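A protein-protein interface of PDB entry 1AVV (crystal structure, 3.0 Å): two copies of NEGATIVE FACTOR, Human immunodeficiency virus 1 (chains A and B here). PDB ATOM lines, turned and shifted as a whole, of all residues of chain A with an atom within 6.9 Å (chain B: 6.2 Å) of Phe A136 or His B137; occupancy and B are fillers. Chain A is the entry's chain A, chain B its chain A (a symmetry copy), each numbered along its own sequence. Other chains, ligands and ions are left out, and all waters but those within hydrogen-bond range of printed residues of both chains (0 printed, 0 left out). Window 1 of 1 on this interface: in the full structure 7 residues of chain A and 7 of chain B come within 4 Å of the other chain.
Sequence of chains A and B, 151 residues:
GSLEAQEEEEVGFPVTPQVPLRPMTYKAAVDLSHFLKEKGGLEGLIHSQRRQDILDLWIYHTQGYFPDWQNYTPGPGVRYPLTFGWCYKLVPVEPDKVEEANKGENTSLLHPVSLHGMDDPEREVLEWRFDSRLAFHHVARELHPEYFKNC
OH of Tyr A26 is in hydrogen-bond range of O of Ala A135, 2.6 Å away.
The side-chain carboxylate (OE1) of Glu A142 is in hydrogen-bond range of a ring nitrogen (NE2) of His A137.
A ring nitrogen (NE2) of His B137 sits at hydrogen-bond distance from the side-chain carboxylate of Glu B142, 2.5 Å away.
A ring nitrogen (ND1) of His B138 is in hydrogen-bond range of the guanidinium group (NE) of Arg B141.
Of the printed residues of chain B, Phe A136 touches Phe B136 (3.4 Å), His B137 (3.6 Å), His B138 (2.9 Å), Arg B141 (3.8 Å) and Glu B142 (3.6 Å).
Printed residues of chain B within 4 Å of Glu A142: Arg B133 and Phe B136.
Ala B135 touches none of the printed residues of chain A.
Printed residues of chain A within 4 Å of Phe B136: Phe A136, His A137, His A138 and Glu A142.
Of chain A, only Arg A133, Phe A136 and His A137 come within 4 Å of His B137.
Of the printed residues of chain A, His B138 touches Phe A136 (2.9 Å).
The nearest residue of chain B that does not touch Phe A136 is Phe B84 (4.6 Å).
The nearest printed residue of chain A that does not touch Arg B133 is Phe A136 (7.0 Å).
The side-chain carboxylate (OE2) of Glu B142 lies within salt-bridge range of the guanidinium group (NE) of Arg A133.
The backbone carbonyl oxygen (O) of Phe A136 sits at hydrogen-bond distance from the backbone NH (N) of His B138.
The backbone carbonyl oxygen (O) of Phe B136 sits at hydrogen-bond distance from the backbone NH (N) of His A138 (2.9 Å).
The side-chain carboxylate of Glu A142 is in salt-bridge range of the guanidinium group of Arg B133, 2.8 Å away.
O of Phe A136 lies close to O of Phe B136 (3.4 Å).
Arg B141 touches Tyr A26.
CG of Arg A133 touches NE2 of His B137, 3.9 Å away.
Phe A136 touches His B137 (O to CA, 3.6 Å).
Phe A136 touches Arg B141.
Phe A136 touches Glu B142 (CD2 to CD, 3.6 Å).
His A137 touches Arg B133 (NE2 to CG, 3.9 Å).
O of Phe B136 touches CA of His A137, 3.6 Å away.
His A137 touches His B137 (CD2 to CB, 3.7 Å).
Glu A142 touches Phe B136 (CD to CD2, 3.6 Å).
Hydrophobic or aromatic side chains of chain A that line the printed part of chain B: Tyr A26, Phe A136, His A137 and His A138.
Of the 13 printed residues of chain B, 6 touch a printed residue of chain A.
Hydrophobic or aromatic side chains of chain B that line the printed part of chain A: Phe B136, His B137 and His B138.
Among the printed residues, Asp or Glu carboxylates within 4 Å of a Lys or Arg side-chain nitrogen of the other chain: Arg A133 with Glu B142 (2.8 Å) and Glu A142 with Arg B133 (2.8 Å).
Arg A133 touches His B137, and with the chains exchanged His A137 touches Arg B133.
Phe B136 touches its own counterpart, Phe A136.
Phe A136 touches Glu B142, and with the chains exchanged Glu A142 touches Phe B136.
His B137 touches its own counterpart, His A137.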
ATOM      1  N   TYR A  26      21.573 -19.865 -32.035  1.00  0.00           N
ATOM      2  CA  TYR A  26      20.798 -20.920 -31.394  1.00  0.00           C
ATOM      3  C   TYR A  26      20.972 -22.217 -32.178  1.00  0.00           C
ATOM      4  O   TYR A  26      21.099 -23.282 -31.576  1.00  0.00           O
ATOM      5  CB  TYR A  26      19.315 -20.539 -31.345  1.00  0.00           C
ATOM      6  CG  TYR A  26      18.343 -21.658 -30.971  1.00  0.00           C
ATOM      7  CD1 TYR A  26      17.915 -22.583 -31.918  1.00  0.00           C
ATOM      8  CD2 TYR A  26      17.831 -21.766 -29.665  1.00  0.00           C
ATOM      9  CE1 TYR A  26      17.018 -23.575 -31.584  1.00  0.00           C
ATOM     10  CE2 TYR A  26      16.928 -22.763 -29.325  1.00  0.00           C
ATOM     11  CZ  TYR A  26      16.532 -23.665 -30.289  1.00  0.00           C
ATOM     12  OH  TYR A  26      15.672 -24.695 -29.963  1.00  0.00           O
ATOM     13  N   PHE A  84      20.879 -19.477 -25.214  1.00  0.00           N
ATOM     14  CA  PHE A  84      19.703 -20.272 -25.496  1.00  0.00           C
ATOM     15  C   PHE A  84      20.087 -21.191 -26.620  1.00  0.00           C
ATOM     16  O   PHE A  84      20.674 -20.753 -27.618  1.00  0.00           O
ATOM     17  CB  PHE A  84      18.551 -19.375 -25.959  1.00  0.00           C
ATOM     18  CG  PHE A  84      17.217 -20.088 -26.051  1.00  0.00           C
ATOM     19  CD1 PHE A  84      16.800 -20.971 -25.036  1.00  0.00           C
ATOM     20  CD2 PHE A  84      16.352 -19.824 -27.089  1.00  0.00           C
ATOM     21  CE1 PHE A  84      15.537 -21.563 -25.065  1.00  0.00           C
ATOM     22  CE2 PHE A  84      15.101 -20.409 -27.121  1.00  0.00           C
ATOM     23  CZ  PHE A  84      14.692 -21.279 -26.104  1.00  0.00           C
ATOM     24  N   GLY A  85      19.750 -22.464 -26.466  1.00  0.00           N
ATOM     25  CA  GLY A  85      20.078 -23.426 -27.497  1.00  0.00           C
ATOM     26  C   GLY A  85      21.024 -24.397 -26.872  1.00  0.00           C
ATOM     27  O   GLY A  85      20.922 -25.585 -27.119  1.00  0.00           O
ATOM     28  N   CYS A  87      22.015 -26.709 -24.375  1.00  0.00           N
ATOM     29  CA  CYS A  87      21.227 -27.510 -23.440  1.00  0.00           C
ATOM     30  C   CYS A  87      22.046 -28.321 -22.447  1.00  0.00           C
ATOM     31  O   CYS A  87      22.080 -29.537 -22.558  1.00  0.00           O
ATOM     32  CB  CYS A  87      20.330 -28.512 -24.192  1.00  0.00           C
ATOM     33  SG  CYS A  87      19.487 -28.005 -25.724  1.00  0.00           S
ATOM     34  N   SER A 132      16.969 -31.216 -22.195  1.00  0.00           N
ATOM     35  CA  SER A 132      16.426 -30.620 -23.432  1.00  0.00           C
ATOM     36  C   SER A 132      15.248 -29.662 -23.364  1.00  0.00           C
ATOM     37  O   SER A 132      14.857 -29.129 -24.407  1.00  0.00           O
ATOM     38  CB  SER A 132      16.189 -31.659 -24.519  1.00  0.00           C
ATOM     39  OG  SER A 132      15.492 -32.759 -23.988  1.00  0.00           O
ATOM     40  N   ARG A 133      14.676 -29.455 -22.169  1.00  0.00           N
ATOM     41  CA  ARG A 133      13.607 -28.481 -22.036  1.00  0.00           C
ATOM     42  C   ARG A 133      14.329 -27.138 -22.061  1.00  0.00           C
ATOM     43  O   ARG A 133      13.694 -26.087 -22.002  1.00  0.00           O
ATOM     44  CB  ARG A 133      12.771 -28.644 -20.755  1.00  0.00           C
ATOM     45  CG  ARG A 133      11.514 -27.714 -20.749  1.00  0.00           C
ATOM     46  CD  ARG A 133      10.331 -28.149 -19.819  1.00  0.00           C
ATOM     47  NE  ARG A 133       9.584 -29.351 -20.263  1.00  0.00           N
ATOM     48  CZ  ARG A 133       8.402 -29.754 -19.774  1.00  0.00           C
ATOM     49  NH1 ARG A 133       7.784 -29.065 -18.824  1.00  0.00           N
ATOM     50  NH2 ARG A 133       7.845 -30.876 -20.211  1.00  0.00           N
ATOM     51  N   LEU A 134      15.661 -27.191 -22.215  1.00  0.00           N
ATOM     52  CA  LEU A 134      16.549 -26.014 -22.270  1.00  0.00           C
ATOM     53  C   LEU A 134      16.676 -25.460 -23.652  1.00  0.00           C
ATOM     54  O   LEU A 134      17.171 -24.342 -23.830  1.00  0.00           O
ATOM     55  CB  LEU A 134      17.958 -26.368 -21.822  1.00  0.00           C
ATOM     56  CG  LEU A 134      18.210 -26.517 -20.326  1.00  0.00           C
ATOM     57  CD1 LEU A 134      19.706 -26.708 -20.157  1.00  0.00           C
ATOM     58  CD2 LEU A 134      17.714 -25.314 -19.534  1.00  0.00           C
ATOM     59  N   ALA A 135      16.360 -26.315 -24.620  1.00  0.00           N
ATOM     60  CA  ALA A 135      16.389 -25.985 -26.038  1.00  0.00           C
ATOM     61  C   ALA A 135      15.122 -25.211 -26.393  1.00  0.00           C
ATOM     62  O   ALA A 135      14.977 -24.714 -27.505  1.00  0.00           O
ATOM     63  CB  ALA A 135      16.442 -27.252 -26.851  1.00  0.00           C
ATOM     64  N   PHE A 136      14.194 -25.127 -25.444  1.00  0.00           N
ATOM     65  CA  PHE A 136      12.940 -24.440 -25.668  1.00  0.00           C
ATOM     66  C   PHE A 136      12.698 -23.420 -24.574  1.00  0.00           C
ATOM     67  O   PHE A 136      12.078 -22.398 -24.812  1.00  0.00           O
ATOM     68  CB  PHE A 136      11.790 -25.440 -25.657  1.00  0.00           C
ATOM     69  CG  PHE A 136      11.989 -26.623 -26.563  1.00  0.00           C
ATOM     70  CD1 PHE A 136      12.289 -26.442 -27.916  1.00  0.00           C
ATOM     71  CD2 PHE A 136      11.952 -27.919 -26.045  1.00  0.00           C
ATOM     72  CE1 PHE A 136      12.566 -27.535 -28.747  1.00  0.00           C
ATOM     73  CE2 PHE A 136      12.226 -29.014 -26.856  1.00  0.00           C
ATOM     74  CZ  PHE A 136      12.539 -28.822 -28.216  1.00  0.00           C
ATOM     75  N   HIS A 137      13.136 -23.713 -23.356  1.00  0.00           N
ATOM     76  CA  HIS A 137      12.928 -22.780 -22.258  1.00  0.00           C
ATOM     77  C   HIS A 137      14.182 -21.987 -21.985  1.00  0.00           C
ATOM     78  O   HIS A 137      15.206 -22.565 -21.593  1.00  0.00           O
ATOM     79  CB  HIS A 137      12.509 -23.517 -20.974  1.00  0.00           C
ATOM     80  CG  HIS A 137      11.938 -22.613 -19.915  1.00  0.00           C
ATOM     81  ND1 HIS A 137      11.593 -23.058 -18.659  1.00  0.00           N
ATOM     82  CD2 HIS A 137      11.607 -21.295 -19.947  1.00  0.00           C
ATOM     83  CE1 HIS A 137      11.068 -22.060 -17.966  1.00  0.00           C
ATOM     84  NE2 HIS A 137      11.063 -20.980 -18.726  1.00  0.00           N
ATOM     85  N   HIS A 138      14.131 -20.674 -22.215  1.00  0.00           N
ATOM     86  CA  HIS A 138      15.305 -19.864 -21.921  1.00  0.00           C
ATOM     87  C   HIS A 138      15.215 -19.524 -20.431  1.00  0.00           C
ATOM     88  O   HIS A 138      14.904 -18.399 -20.034  1.00  0.00           O
ATOM     89  CB  HIS A 138      15.393 -18.604 -22.776  1.00  0.00           C
ATOM     90  CG  HIS A 138      16.780 -18.017 -22.821  1.00  0.00           C
ATOM     91  ND1 HIS A 138      17.024 -16.661 -22.916  1.00  0.00           N
ATOM     92  CD2 HIS A 138      17.997 -18.612 -22.762  1.00  0.00           C
ATOM     93  CE1 HIS A 138      18.329 -16.454 -22.912  1.00  0.00           C
ATOM     94  NE2 HIS A 138      18.940 -17.621 -22.818  1.00  0.00           N
ATOM     95  N   VAL A 139      15.531 -20.524 -19.606  1.00  0.00           N
ATOM     96  CA  VAL A 139      15.450 -20.380 -18.164  1.00  0.00           C
ATOM     97  C   VAL A 139      16.246 -19.204 -17.688  1.00  0.00           C
ATOM     98  O   VAL A 139      15.674 -18.265 -17.191  1.00  0.00           O
ATOM     99  CB  VAL A 139      15.942 -21.608 -17.424  1.00  0.00           C
ATOM    100  CG1 VAL A 139      15.448 -21.530 -15.995  1.00  0.00           C
ATOM    101  CG2 VAL A 139      15.475 -22.881 -18.102  1.00  0.00           C
ATOM    102  N   GLU A 142      14.713 -16.080 -17.862  1.00  0.00           N
ATOM    103  CA  GLU A 142      13.546 -15.955 -17.007  1.00  0.00           C
ATOM    104  C   GLU A 142      13.964 -15.471 -15.625  1.00  0.00           C
ATOM    105  O   GLU A 142      13.400 -14.490 -15.133  1.00  0.00           O
ATOM    106  CB  GLU A 142      12.753 -17.271 -16.919  1.00  0.00           C
ATOM    107  CG  GLU A 142      11.503 -17.165 -16.037  1.00  0.00           C
ATOM    108  CD  GLU A 142      10.356 -18.096 -16.432  1.00  0.00           C
ATOM    109  OE1 GLU A 142      10.499 -18.887 -17.389  1.00  0.00           O
ATOM    110  OE2 GLU A 142       9.295 -18.008 -15.776  1.00  0.00           O
ATOM    111  N   PHE B  84       7.241 -17.174 -30.999  1.00  0.00           N
ATOM    112  CA  PHE B  84       7.883 -17.018 -29.711  1.00  0.00           C
ATOM    113  C   PHE B  84       7.967 -15.539 -29.468  1.00  0.00           C
ATOM    114  O   PHE B  84       8.381 -14.779 -30.355  1.00  0.00           O
ATOM    115  CB  PHE B  84       9.300 -17.598 -29.747  1.00  0.00           C
ATOM    116  CG  PHE B  84       9.959 -17.692 -28.386  1.00  0.00           C
ATOM    117  CD1 PHE B  84       9.242 -18.164 -27.269  1.00  0.00           C
ATOM    118  CD2 PHE B  84      11.295 -17.394 -28.232  1.00  0.00           C
ATOM    119  CE1 PHE B  84       9.864 -18.341 -26.032  1.00  0.00           C
ATOM    120  CE2 PHE B  84      11.912 -17.566 -27.009  1.00  0.00           C
ATOM    121  CZ  PHE B  84      11.194 -18.044 -25.907  1.00  0.00           C
ATOM    122  N   SER B 132       3.234 -14.904 -19.124  1.00  0.00           N
ATOM    123  CA  SER B 132       4.614 -14.499 -19.462  1.00  0.00           C
ATOM    124  C   SER B 132       5.738 -15.522 -19.429  1.00  0.00           C
ATOM    125  O   SER B 132       6.869 -15.170 -19.778  1.00  0.00           O
ATOM    126  CB  SER B 132       5.040 -13.234 -18.731  1.00  0.00           C
ATOM    127  OG  SER B 132       4.728 -13.341 -17.363  1.00  0.00           O
ATOM    128  N   ARG B 133       5.448 -16.759 -19.002  1.00  0.00           N
ATOM    129  CA  ARG B 133       6.465 -17.795 -19.038  1.00  0.00           C
ATOM    130  C   ARG B 133       6.539 -18.187 -20.510  1.00  0.00           C
ATOM    131  O   ARG B 133       7.346 -19.033 -20.891  1.00  0.00           O
ATOM    132  CB  ARG B 133       6.148 -19.011 -18.151  1.00  0.00           C
ATOM    133  CG  ARG B 133       7.353 -20.004 -18.059  1.00  0.00           C
ATOM    134  CD  ARG B 133       7.379 -20.953 -16.812  1.00  0.00           C
ATOM    135  NE  ARG B 133       7.674 -20.291 -15.518  1.00  0.00           N
ATOM    136  CZ  ARG B 133       7.991 -20.924 -14.378  1.00  0.00           C
ATOM    137  NH1 ARG B 133       8.079 -22.246 -14.332  1.00  0.00           N
ATOM    138  NH2 ARG B 133       8.187 -20.234 -13.263  1.00  0.00           N
ATOM    139  N   LEU B 134       5.729 -17.509 -21.339  1.00  0.00           N
ATOM    140  CA  LEU B 134       5.645 -17.724 -22.796  1.00  0.00           C
ATOM    141  C   LEU B 134       6.653 -16.920 -23.550  1.00  0.00           C
ATOM    142  O   LEU B 134       6.884 -17.170 -24.738  1.00  0.00           O
ATOM    143  CB  LEU B 134       4.284 -17.313 -23.333  1.00  0.00           C
ATOM    144  CG  LEU B 134       3.114 -18.263 -23.103  1.00  0.00           C
ATOM    145  CD1 LEU B 134       1.936 -17.691 -23.870  1.00  0.00           C
ATOM    146  CD2 LEU B 134       3.427 -19.685 -23.550  1.00  0.00           C
ATOM    147  N   ALA B 135       7.131 -15.871 -22.886  1.00  0.00           N
ATOM    148  CA  ALA B 135       8.139 -14.963 -23.416  1.00  0.00           C
ATOM    149  C   ALA B 135       9.515 -15.607 -23.266  1.00  0.00           C
ATOM    150  O   ALA B 135      10.512 -15.085 -23.757  1.00  0.00           O
ATOM    151  CB  ALA B 135       8.107 -13.669 -22.645  1.00  0.00           C
ATOM    152  N   PHE B 136       9.567 -16.737 -22.569  1.00  0.00           N
ATOM    153  CA  PHE B 136      10.817 -17.429 -22.339  1.00  0.00           C
ATOM    154  C   PHE B 136      10.698 -18.882 -22.752  1.00  0.00           C
ATOM    155  O   PHE B 136      11.670 -19.483 -23.176  1.00  0.00           O
ATOM    156  CB  PHE B 136      11.174 -17.378 -20.858  1.00  0.00           C
ATOM    157  CG  PHE B 136      11.140 -15.998 -20.259  1.00  0.00           C
ATOM    158  CD1 PHE B 136      11.865 -14.952 -20.836  1.00  0.00           C
ATOM    159  CD2 PHE B 136      10.318 -15.729 -19.162  1.00  0.00           C
ATOM    160  CE1 PHE B 136      11.767 -13.646 -20.341  1.00  0.00           C
ATOM    161  CE2 PHE B 136      10.209 -14.438 -18.660  1.00  0.00           C
ATOM    162  CZ  PHE B 136      10.934 -13.387 -19.255  1.00  0.00           C
ATOM    163  N   HIS B 137       9.521 -19.471 -22.581  1.00  0.00           N
ATOM    164  CA  HIS B 137       9.342 -20.868 -22.949  1.00  0.00           C
ATOM    165  C   HIS B 137       8.653 -20.985 -24.287  1.00  0.00           C
ATOM    166  O   HIS B 137       7.494 -20.569 -24.424  1.00  0.00           O
ATOM    167  CB  HIS B 137       8.516 -21.621 -21.891  1.00  0.00           C
ATOM    168  CG  HIS B 137       8.590 -23.119 -22.017  1.00  0.00           C
ATOM    169  ND1 HIS B 137       7.849 -23.972 -21.230  1.00  0.00           N
ATOM    170  CD2 HIS B 137       9.359 -23.914 -22.807  1.00  0.00           C
ATOM    171  CE1 HIS B 137       8.162 -25.224 -21.522  1.00  0.00           C
ATOM    172  NE2 HIS B 137       9.077 -25.215 -22.476  1.00  0.00           N
ATOM    173  N   HIS B 138       9.358 -21.515 -25.287  1.00  0.00           N
ATOM    174  CA  HIS B 138       8.717 -21.688 -26.583  1.00  0.00           C
ATOM    175  C   HIS B 138       7.974 -23.024 -26.507  1.00  0.00           C
ATOM    176  O   HIS B 138       8.382 -24.034 -27.084  1.00  0.00           O
ATOM    177  CB  HIS B 138       9.703 -21.664 -27.747  1.00  0.00           C
ATOM    178  CG  HIS B 138       9.044 -21.381 -29.072  1.00  0.00           C
ATOM    179  ND1 HIS B 138       9.485 -21.917 -30.266  1.00  0.00           N
ATOM    180  CD2 HIS B 138       7.959 -20.628 -29.380  1.00  0.00           C
ATOM    181  CE1 HIS B 138       8.698 -21.505 -31.244  1.00  0.00           C
ATOM    182  NE2 HIS B 138       7.764 -20.723 -30.731  1.00  0.00           N
ATOM    183  N   VAL B 139       6.843 -22.999 -25.798  1.00  0.00           N
ATOM    184  CA  VAL B 139       6.046 -24.194 -25.588  1.00  0.00           C
ATOM    185  C   VAL B 139       5.688 -24.846 -26.888  1.00  0.00           C
ATOM    186  O   VAL B 139       6.132 -25.939 -27.143  1.00  0.00           O
ATOM    187  CB  VAL B 139       4.760 -23.915 -24.835  1.00  0.00           C
ATOM    188  CG1 VAL B 139       4.219 -25.231 -24.317  1.00  0.00           C
ATOM    189  CG2 VAL B 139       4.988 -22.928 -23.707  1.00  0.00           C
ATOM    190  N   ALA B 140       4.918 -24.149 -27.722  1.00  0.00           N
ATOM    191  CA  ALA B 140       4.492 -24.665 -29.028  1.00  0.00           C
ATOM    192  C   ALA B 140       5.574 -25.405 -29.811  1.00  0.00           C
ATOM    193  O   ALA B 140       5.246 -26.326 -30.558  1.00  0.00           O
ATOM    194  CB  ALA B 140       3.906 -23.560 -29.875  1.00  0.00           C
ATOM    195  N   ARG B 141       6.839 -24.990 -29.704  1.00  0.00           N
ATOM    196  CA  ARG B 141       7.868 -25.742 -30.405  1.00  0.00           C
ATOM    197  C   ARG B 141       8.185 -27.005 -29.631  1.00  0.00           C
ATOM    198  O   ARG B 141       8.554 -28.009 -30.220  1.00  0.00           O
ATOM    199  CB  ARG B 141       9.159 -24.978 -30.634  1.00  0.00           C
ATOM    200  CG  ARG B 141      10.207 -25.898 -31.245  1.00  0.00           C
ATOM    201  CD  ARG B 141      11.349 -25.149 -31.837  1.00  0.00           C
ATOM    202  NE  ARG B 141      11.666 -23.988 -31.013  1.00  0.00           N
ATOM    203  CZ  ARG B 141      12.610 -23.097 -31.314  1.00  0.00           C
ATOM    204  NH1 ARG B 141      13.335 -23.270 -32.431  1.00  0.00           N
ATOM    205  NH2 ARG B 141      12.779 -22.009 -30.542  1.00  0.00           N
ATOM    206  N   GLU B 142       8.069 -26.956 -28.309  1.00  0.00           N
ATOM    207  CA  GLU B 142       8.356 -28.133 -27.509  1.00  0.00           C
ATOM    208  C   GLU B 142       7.401 -29.259 -27.881  1.00  0.00           C
ATOM    209  O   GLU B 142       7.859 -30.366 -28.174  1.00  0.00           O
ATOM    210  CB  GLU B 142       8.301 -27.832 -26.001  1.00  0.00           C
ATOM    211  CG  GLU B 142       8.618 -29.052 -25.129  1.00  0.00           C
ATOM    212  CD  GLU B 142       9.257 -28.730 -23.778  1.00  0.00           C
ATOM    213  OE1 GLU B 142       9.448 -27.539 -23.449  1.00  0.00           O
ATOM    214  OE2 GLU B 142       9.584 -29.696 -23.053  1.00  0.00           O
ATOM    215  N   PRO B 145       7.124 -30.074 -32.682  1.00  0.00           N
ATOM    216  CA  PRO B 145       8.387 -29.744 -33.376  1.00  0.00           C
ATOM    217  C   PRO B 145       8.263 -29.748 -34.902  1.00  0.00           C
ATOM    218  O   PRO B 145       9.065 -29.117 -35.606  1.00  0.00           O
ATOM    219  CB  PRO B 145       9.354 -30.838 -32.889  1.00  0.00           C
ATOM    220  CG  PRO B 145       8.766 -31.277 -31.548  1.00  0.00           C
ATOM    221  CD  PRO B 145       7.275 -31.276 -31.837  1.00  0.00           C
